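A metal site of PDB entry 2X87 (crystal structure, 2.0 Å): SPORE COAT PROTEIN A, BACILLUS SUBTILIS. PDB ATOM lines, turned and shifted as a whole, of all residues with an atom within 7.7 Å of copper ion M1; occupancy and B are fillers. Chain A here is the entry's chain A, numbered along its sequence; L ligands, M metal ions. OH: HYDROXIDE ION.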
ATOM      1  N   HIS A 105      22.893  21.164   5.236  1.00  0.00           N
ATOM      2  CA  HIS A 105      22.624  20.524   6.496  1.00  0.00           C
ATOM      3  C   HIS A 105      22.765  19.002   6.369  1.00  0.00           C
ATOM      4  O   HIS A 105      22.133  18.390   5.507  1.00  0.00           O
ATOM      5  CB  HIS A 105      21.232  20.878   6.974  1.00  0.00           C
ATOM      6  CG  HIS A 105      20.766  20.027   8.113  1.00  0.00           C
ATOM      7  ND1 HIS A 105      21.412  20.004   9.334  1.00  0.00           N
ATOM      8  CD2 HIS A 105      19.745  19.156   8.206  1.00  0.00           C
ATOM      9  CE1 HIS A 105      20.786  19.156  10.132  1.00  0.00           C
ATOM     10  NE2 HIS A 105      19.774  18.626   9.474  1.00  0.00           N
ATOM     11  N   LEU A 106      23.607  18.433   7.221  1.00  0.00           N
ATOM     12  CA  LEU A 106      23.709  16.978   7.372  1.00  0.00           C
ATOM     13  C   LEU A 106      22.651  16.514   8.372  1.00  0.00           C
ATOM     14  O   LEU A 106      22.826  16.617   9.586  1.00  0.00           O
ATOM     15  CB  LEU A 106      25.118  16.552   7.822  1.00  0.00           C
ATOM     16  CG  LEU A 106      25.348  15.034   7.973  1.00  0.00           C
ATOM     17  CD1 LEU A 106      25.066  14.312   6.645  1.00  0.00           C
ATOM     18  CD2 LEU A 106      26.764  14.732   8.456  1.00  0.00           C
ATOM     19  N   HIS A 107      21.556  16.003   7.818  1.00  0.00           N
ATOM     20  CA  HIS A 107      20.406  15.576   8.579  1.00  0.00           C
ATOM     21  C   HIS A 107      20.726  14.329   9.378  1.00  0.00           C
ATOM     22  O   HIS A 107      21.095  13.298   8.803  1.00  0.00           O
ATOM     23  CB  HIS A 107      19.234  15.343   7.627  1.00  0.00           C
ATOM     24  CG  HIS A 107      17.924  15.130   8.322  1.00  0.00           C
ATOM     25  ND1 HIS A 107      16.863  16.001   8.205  1.00  0.00           N
ATOM     26  CD2 HIS A 107      17.514  14.146   9.163  1.00  0.00           C
ATOM     27  CE1 HIS A 107      15.855  15.555   8.932  1.00  0.00           C
ATOM     28  NE2 HIS A 107      16.224  14.430   9.519  1.00  0.00           N
ATOM     29  N   GLY A 108      20.606  14.441  10.699  1.00  0.00           N
ATOM     30  CA  GLY A 108      20.988  13.378  11.628  1.00  0.00           C
ATOM     31  C   GLY A 108      22.424  13.501  12.150  1.00  0.00           C
ATOM     32  O   GLY A 108      22.853  12.713  12.996  1.00  0.00           O
ATOM     33  N   TRP A 151      21.365  11.955   5.612  1.00  0.00           N
ATOM     34  CA  TRP A 151      21.275  12.544   4.282  1.00  0.00           C
ATOM     35  C   TRP A 151      21.548  14.021   4.384  1.00  0.00           C
ATOM     36  O   TRP A 151      21.374  14.610   5.435  1.00  0.00           O
ATOM     37  CB  TRP A 151      19.927  12.222   3.600  1.00  0.00           C
ATOM     38  CG  TRP A 151      18.697  12.881   4.183  1.00  0.00           C
ATOM     39  CD1 TRP A 151      18.171  12.705   5.434  1.00  0.00           C
ATOM     40  CD2 TRP A 151      17.805  13.780   3.496  1.00  0.00           C
ATOM     41  NE1 TRP A 151      17.025  13.449   5.577  1.00  0.00           N
ATOM     42  CE2 TRP A 151      16.767  14.119   4.406  1.00  0.00           C
ATOM     43  CE3 TRP A 151      17.775  14.339   2.206  1.00  0.00           C
ATOM     44  CZ2 TRP A 151      15.724  14.994   4.067  1.00  0.00           C
ATOM     45  CZ3 TRP A 151      16.737  15.205   1.869  1.00  0.00           C
ATOM     46  CH2 TRP A 151      15.725  15.526   2.797  1.00  0.00           C
ATOM     47  N   TYR A 152      22.036  14.613   3.303  1.00  0.00           N
ATOM     48  CA  TYR A 152      22.382  16.018   3.338  1.00  0.00           C
ATOM     49  C   TYR A 152      21.554  16.744   2.304  1.00  0.00           C
ATOM     50  O   TYR A 152      21.195  16.195   1.251  1.00  0.00           O
ATOM     51  CB  TYR A 152      23.888  16.249   3.152  1.00  0.00           C
ATOM     52  CG  TYR A 152      24.466  15.736   1.845  1.00  0.00           C
ATOM     53  CD1 TYR A 152      24.560  16.578   0.742  1.00  0.00           C
ATOM     54  CD2 TYR A 152      24.911  14.414   1.716  1.00  0.00           C
ATOM     55  CE1 TYR A 152      25.080  16.117  -0.464  1.00  0.00           C
ATOM     56  CE2 TYR A 152      25.435  13.944   0.512  1.00  0.00           C
ATOM     57  CZ  TYR A 152      25.516  14.806  -0.574  1.00  0.00           C
ATOM     58  OH  TYR A 152      26.019  14.384  -1.775  1.00  0.00           O
ATOM     59  N   HIS A 153      21.215  17.983   2.638  1.00  0.00           N
ATOM     60  CA  HIS A 153      20.329  18.775   1.818  1.00  0.00           C
ATOM     61  C   HIS A 153      20.472  20.254   2.149  1.00  0.00           C
ATOM     62  O   HIS A 153      20.994  20.611   3.212  1.00  0.00           O
ATOM     63  CB  HIS A 153      18.857  18.308   1.940  1.00  0.00           C
ATOM     64  CG  HIS A 153      18.262  18.456   3.315  1.00  0.00           C
ATOM     65  ND1 HIS A 153      17.721  19.637   3.768  1.00  0.00           N
ATOM     66  CD2 HIS A 153      18.083  17.548   4.310  1.00  0.00           C
ATOM     67  CE1 HIS A 153      17.266  19.468   4.997  1.00  0.00           C
ATOM     68  NE2 HIS A 153      17.463  18.207   5.354  1.00  0.00           N
ATOM     69  N   ASP A 154      20.019  21.104   1.231  1.00  0.00           N
ATOM     70  CA  ASP A 154      20.040  22.540   1.479  1.00  0.00           C
ATOM     71  C   ASP A 154      19.098  22.923   2.627  1.00  0.00           C
ATOM     72  O   ASP A 154      18.048  22.318   2.806  1.00  0.00           O
ATOM     73  CB  ASP A 154      19.662  23.302   0.219  1.00  0.00           C
ATOM     74  CG  ASP A 154      19.943  24.780   0.364  1.00  0.00           C
ATOM     75  OD1 ASP A 154      18.982  25.528   0.632  1.00  0.00           O
ATOM     76  OD2 ASP A 154      21.115  25.158   0.274  1.00  0.00           O
ATOM     77  N   HIS A 155      19.490  23.942   3.399  1.00  0.00           N
ATOM     78  CA  HIS A 155      18.695  24.384   4.550  1.00  0.00           C
ATOM     79  C   HIS A 155      18.611  25.933   4.622  1.00  0.00           C
ATOM     80  O   HIS A 155      18.360  26.489   5.688  1.00  0.00           O
ATOM     81  CB  HIS A 155      19.327  23.833   5.860  1.00  0.00           C
ATOM     82  CG  HIS A 155      18.337  23.441   6.931  1.00  0.00           C
ATOM     83  ND1 HIS A 155      17.482  24.325   7.529  1.00  0.00           N
ATOM     84  CD2 HIS A 155      18.123  22.247   7.542  1.00  0.00           C
ATOM     85  CE1 HIS A 155      16.767  23.701   8.451  1.00  0.00           C
ATOM     86  NE2 HIS A 155      17.132  22.434   8.481  1.00  0.00           N
ATOM     87  N   THR A 160      14.483  26.809   1.376  1.00  0.00           N
ATOM     88  CA  THR A 160      14.691  25.361   1.533  1.00  0.00           C
ATOM     89  C   THR A 160      13.811  24.513   0.597  1.00  0.00           C
ATOM     90  O   THR A 160      14.318  23.595  -0.062  1.00  0.00           O
ATOM     91  CB  THR A 160      14.541  24.943   3.019  1.00  0.00           C
ATOM     92  OG1 THR A 160      15.555  25.591   3.792  1.00  0.00           O
ATOM     93  CG2 THR A 160      14.678  23.431   3.190  1.00  0.00           C
ATOM     94  N   VAL A 164      15.922  22.355  -2.322  1.00  0.00           N
ATOM     95  CA  VAL A 164      15.806  20.907  -2.230  1.00  0.00           C
ATOM     96  C   VAL A 164      15.066  20.360  -3.475  1.00  0.00           C
ATOM     97  O   VAL A 164      15.526  19.411  -4.123  1.00  0.00           O
ATOM     98  CB  VAL A 164      15.110  20.460  -0.924  1.00  0.00           C
ATOM     99  CG1 VAL A 164      14.752  18.960  -0.954  1.00  0.00           C
ATOM    100  CG2 VAL A 164      16.005  20.782   0.297  1.00  0.00           C
ATOM    101  N   ASN A 256      13.204   9.372   2.530  1.00  0.00           N
ATOM    102  CA  ASN A 256      12.210  10.255   1.929  1.00  0.00           C
ATOM    103  C   ASN A 256      12.785  11.676   1.759  1.00  0.00           C
ATOM    104  O   ASN A 256      12.877  12.438   2.716  1.00  0.00           O
ATOM    105  CB  ASN A 256      10.896  10.278   2.723  1.00  0.00           C
ATOM    106  CG  ASN A 256       9.804  11.118   2.044  1.00  0.00           C
ATOM    107  OD1 ASN A 256      10.083  11.917   1.159  1.00  0.00           O
ATOM    108  ND2 ASN A 256       8.566  10.937   2.484  1.00  0.00           N
ATOM    109  N   PRO A 296       8.365  12.944   5.032  1.00  0.00           N
ATOM    110  CA  PRO A 296       9.607  13.645   4.682  1.00  0.00           C
ATOM    111  C   PRO A 296      10.699  13.576   5.764  1.00  0.00           C
ATOM    112  O   PRO A 296      10.414  13.794   6.952  1.00  0.00           O
ATOM    113  CB  PRO A 296       9.150  15.088   4.479  1.00  0.00           C
ATOM    114  CG  PRO A 296       7.745  14.939   3.976  1.00  0.00           C
ATOM    115  CD  PRO A 296       7.173  13.740   4.710  1.00  0.00           C
ATOM    116  N   ALA A 297      11.917  13.262   5.326  1.00  0.00           N
ATOM    117  CA  ALA A 297      13.150  13.189   6.150  1.00  0.00           C
ATOM    118  C   ALA A 297      13.308  11.919   6.988  1.00  0.00           C
ATOM    119  O   ALA A 297      14.381  11.688   7.550  1.00  0.00           O
ATOM    120  CB  ALA A 297      13.341  14.431   7.024  1.00  0.00           C
ATOM    121  N   ARG A 299      13.933   7.947   7.600  1.00  0.00           N
ATOM    122  CA  ARG A 299      14.724   6.918   6.950  1.00  0.00           C
ATOM    123  C   ARG A 299      14.374   5.548   7.514  1.00  0.00           C
ATOM    124  O   ARG A 299      14.210   5.389   8.735  1.00  0.00           O
ATOM    125  CB  ARG A 299      16.234   7.162   7.104  1.00  0.00           C
ATOM    126  CG  ARG A 299      16.792   8.325   6.293  1.00  0.00           C
ATOM    127  CD  ARG A 299      16.731   9.647   7.054  1.00  0.00           C
ATOM    128  NE  ARG A 299      17.721   9.688   8.137  1.00  0.00           N
ATOM    129  CZ  ARG A 299      17.612  10.422   9.241  1.00  0.00           C
ATOM    130  NH1 ARG A 299      16.546  11.182   9.433  1.00  0.00           N
ATOM    131  NH2 ARG A 299      18.566  10.387  10.164  1.00  0.00           N
ATOM    132  N   HIS A 422      11.217  17.447  13.302  1.00  0.00           N
ATOM    133  CA  HIS A 422      12.625  17.127  13.328  1.00  0.00           C
ATOM    134  C   HIS A 422      13.370  17.997  14.341  1.00  0.00           C
ATOM    135  O   HIS A 422      13.228  19.222  14.357  1.00  0.00           O
ATOM    136  CB  HIS A 422      13.219  17.278  11.924  1.00  0.00           C
ATOM    137  CG  HIS A 422      14.692  17.052  11.884  1.00  0.00           C
ATOM    138  ND1 HIS A 422      15.284  15.928  12.410  1.00  0.00           N
ATOM    139  CD2 HIS A 422      15.695  17.810  11.390  1.00  0.00           C
ATOM    140  CE1 HIS A 422      16.589  16.000  12.244  1.00  0.00           C
ATOM    141  NE2 HIS A 422      16.869  17.135  11.637  1.00  0.00           N
ATOM    142  N   HIS A 424      17.270  18.919  15.461  1.00  0.00           N
ATOM    143  CA  HIS A 424      18.667  18.831  15.045  1.00  0.00           C
ATOM    144  C   HIS A 424      19.538  18.285  16.182  1.00  0.00           C
ATOM    145  O   HIS A 424      19.110  18.257  17.336  1.00  0.00           O
ATOM    146  CB  HIS A 424      19.171  20.198  14.543  1.00  0.00           C
ATOM    147  CG  HIS A 424      18.686  20.543  13.167  1.00  0.00           C
ATOM    148  ND1 HIS A 424      19.497  21.153  12.227  1.00  0.00           N
ATOM    149  CD2 HIS A 424      17.485  20.365  12.561  1.00  0.00           C
ATOM    150  CE1 HIS A 424      18.813  21.328  11.109  1.00  0.00           C
ATOM    151  NE2 HIS A 424      17.585  20.864  11.285  1.00  0.00           N
ATOM    152  N   ASP A 465      14.909  10.777  14.728  1.00  0.00           N
ATOM    153  CA  ASP A 465      15.186  12.226  14.705  1.00  0.00           C
ATOM    154  C   ASP A 465      14.105  13.039  13.981  1.00  0.00           C
ATOM    155  O   ASP A 465      14.065  14.265  14.084  1.00  0.00           O
ATOM    156  CB  ASP A 465      16.610  12.553  14.220  1.00  0.00           C
ATOM    157  CG  ASP A 465      16.875  12.170  12.748  1.00  0.00           C
ATOM    158  OD1 ASP A 465      15.994  12.364  11.873  1.00  0.00           O
ATOM    159  OD2 ASP A 465      18.003  11.713  12.464  1.00  0.00           O
ATOM    160  N   THR A 466      13.241  12.339  13.262  1.00  0.00           N
ATOM    161  CA  THR A 466      12.133  12.947  12.544  1.00  0.00           C
ATOM    162  C   THR A 466      10.907  12.094  12.838  1.00  0.00           C
ATOM    163  O   THR A 466      10.897  10.901  12.539  1.00  0.00           O
ATOM    164  CB  THR A 466      12.391  13.022  11.009  1.00  0.00           C
ATOM    165  OG1 THR A 466      13.633  13.711  10.757  1.00  0.00           O
ATOM    166  CG2 THR A 466      11.263  13.768  10.292  1.00  0.00           C
ATOM    167  N   HIS A 491      12.085  21.836  13.776  1.00  0.00           N
ATOM    168  CA  HIS A 491      11.140  22.261  12.757  1.00  0.00           C
ATOM    169  C   HIS A 491      10.310  21.116  12.197  1.00  0.00           C
ATOM    170  O   HIS A 491      10.632  19.943  12.382  1.00  0.00           O
ATOM    171  CB  HIS A 491      11.852  22.986  11.596  1.00  0.00           C
ATOM    172  CG  HIS A 491      12.896  22.176  10.884  1.00  0.00           C
ATOM    173  ND1 HIS A 491      12.644  21.494   9.719  1.00  0.00           N
ATOM    174  CD2 HIS A 491      14.202  21.966  11.159  1.00  0.00           C
ATOM    175  CE1 HIS A 491      13.741  20.891   9.307  1.00  0.00           C
ATOM    176  NE2 HIS A 491      14.709  21.175  10.166  1.00  0.00           N
ATOM    177  N   HIS A 493       9.395  19.076   8.962  1.00  0.00           N
ATOM    178  CA  HIS A 493      10.187  18.772   7.775  1.00  0.00           C
ATOM    179  C   HIS A 493       9.347  18.710   6.489  1.00  0.00           C
ATOM    180  O   HIS A 493       9.830  18.280   5.446  1.00  0.00           O
ATOM    181  CB  HIS A 493      11.076  17.520   7.969  1.00  0.00           C
ATOM    182  CG  HIS A 493      12.434  17.642   7.324  1.00  0.00           C
ATOM    183  ND1 HIS A 493      12.605  17.645   5.954  1.00  0.00           N
ATOM    184  CD2 HIS A 493      13.670  17.765   7.861  1.00  0.00           C
ATOM    185  CE1 HIS A 493      13.890  17.773   5.679  1.00  0.00           C
ATOM    186  NE2 HIS A 493      14.564  17.847   6.820  1.00  0.00           N
ATOM    187  N   LEU A 495       8.672  20.926   3.860  1.00  0.00           N
ATOM    188  CA  LEU A 495       9.483  22.076   3.496  1.00  0.00           C
ATOM    189  C   LEU A 495       8.666  23.340   3.257  1.00  0.00           C
ATOM    190  O   LEU A 495       9.101  24.441   3.608  1.00  0.00           O
ATOM    191  CB  LEU A 495      10.398  21.739   2.309  1.00  0.00           C
ATOM    192  CG  LEU A 495      11.369  20.570   2.547  1.00  0.00           C
ATOM    193  CD1 LEU A 495      12.339  20.482   1.393  1.00  0.00           C
ATOM    194  CD2 LEU A 495      12.119  20.681   3.886  1.00  0.00           C
ATOM    195  N   GLU A 498       8.068  24.468   6.830  1.00  0.00           N
ATOM    196  CA  GLU A 498       9.343  24.938   7.375  1.00  0.00           C
ATOM    197  C   GLU A 498       9.673  26.374   6.940  1.00  0.00           C
ATOM    198  O   GLU A 498      10.130  27.175   7.758  1.00  0.00           O
ATOM    199  CB  GLU A 498      10.460  23.988   6.936  1.00  0.00           C
ATOM    200  CG  GLU A 498      11.858  24.380   7.376  1.00  0.00           C
ATOM    201  CD  GLU A 498      12.906  23.379   6.956  1.00  0.00           C
ATOM    202  OE1 GLU A 498      12.585  22.173   6.801  1.00  0.00           O
ATOM    203  OE2 GLU A 498      14.066  23.791   6.798  1.00  0.00           O
HETATM  204  O    OH L   1      16.592  19.213   8.275  1.00  0.00           O
HETATM  205 CU    CU M   1      16.557  17.602   7.048  1.00  0.00          CU
HETATM  206 CU    CU M   2      18.317  17.972  10.620  1.00  0.00          CU
HETATM  207 CU    CU M   3      16.572  20.783   9.532  1.00  0.00          CU
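Copper ion M1 is bound by a ring nitrogen (ND1) of His 107, at 2.0 Å.
Copper ion M1 is bound by a ring nitrogen (NE2) of His 153 (2.0 Å).
Copper ion M1 is bound by a ring nitrogen (NE2) of His 493 (2.0 Å).
O of the ligand is bound to copper ion M1, at 2.0 Å.
Copper ion M1 has four donor atoms within binding distance.
CD2 of His 105 touches copper ion M1, 3.7 Å away.
The nearest printed residue that does not touch copper ion M1 is Trp 151 (4.05 Å).
A ring nitrogen (NE2) of His 107 lies within hydrogen-bond range of the side-chain hydroxyl of Thr 466 (3.0 Å).
A ring nitrogen (NE2) of His 107 lies close to a ring nitrogen (ND1) of His 422, at 3.4 Å.
OD1 of Asp 465 lies within hydrogen-bond range of NE2 of His 107 (3.1 Å).
The backbone carbonyl oxygen (O) of His 153 is in hydrogen-bond range of the backbone NH (N) of His 105, 2.8 Å away.
The backbone NH of His 107 lies within hydrogen-bond range of the backbone carbonyl oxygen of Trp 151, at 2.8 Å.
NH1 of Arg 299 sits close to NE2 of His 107, at 3.3 Å.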
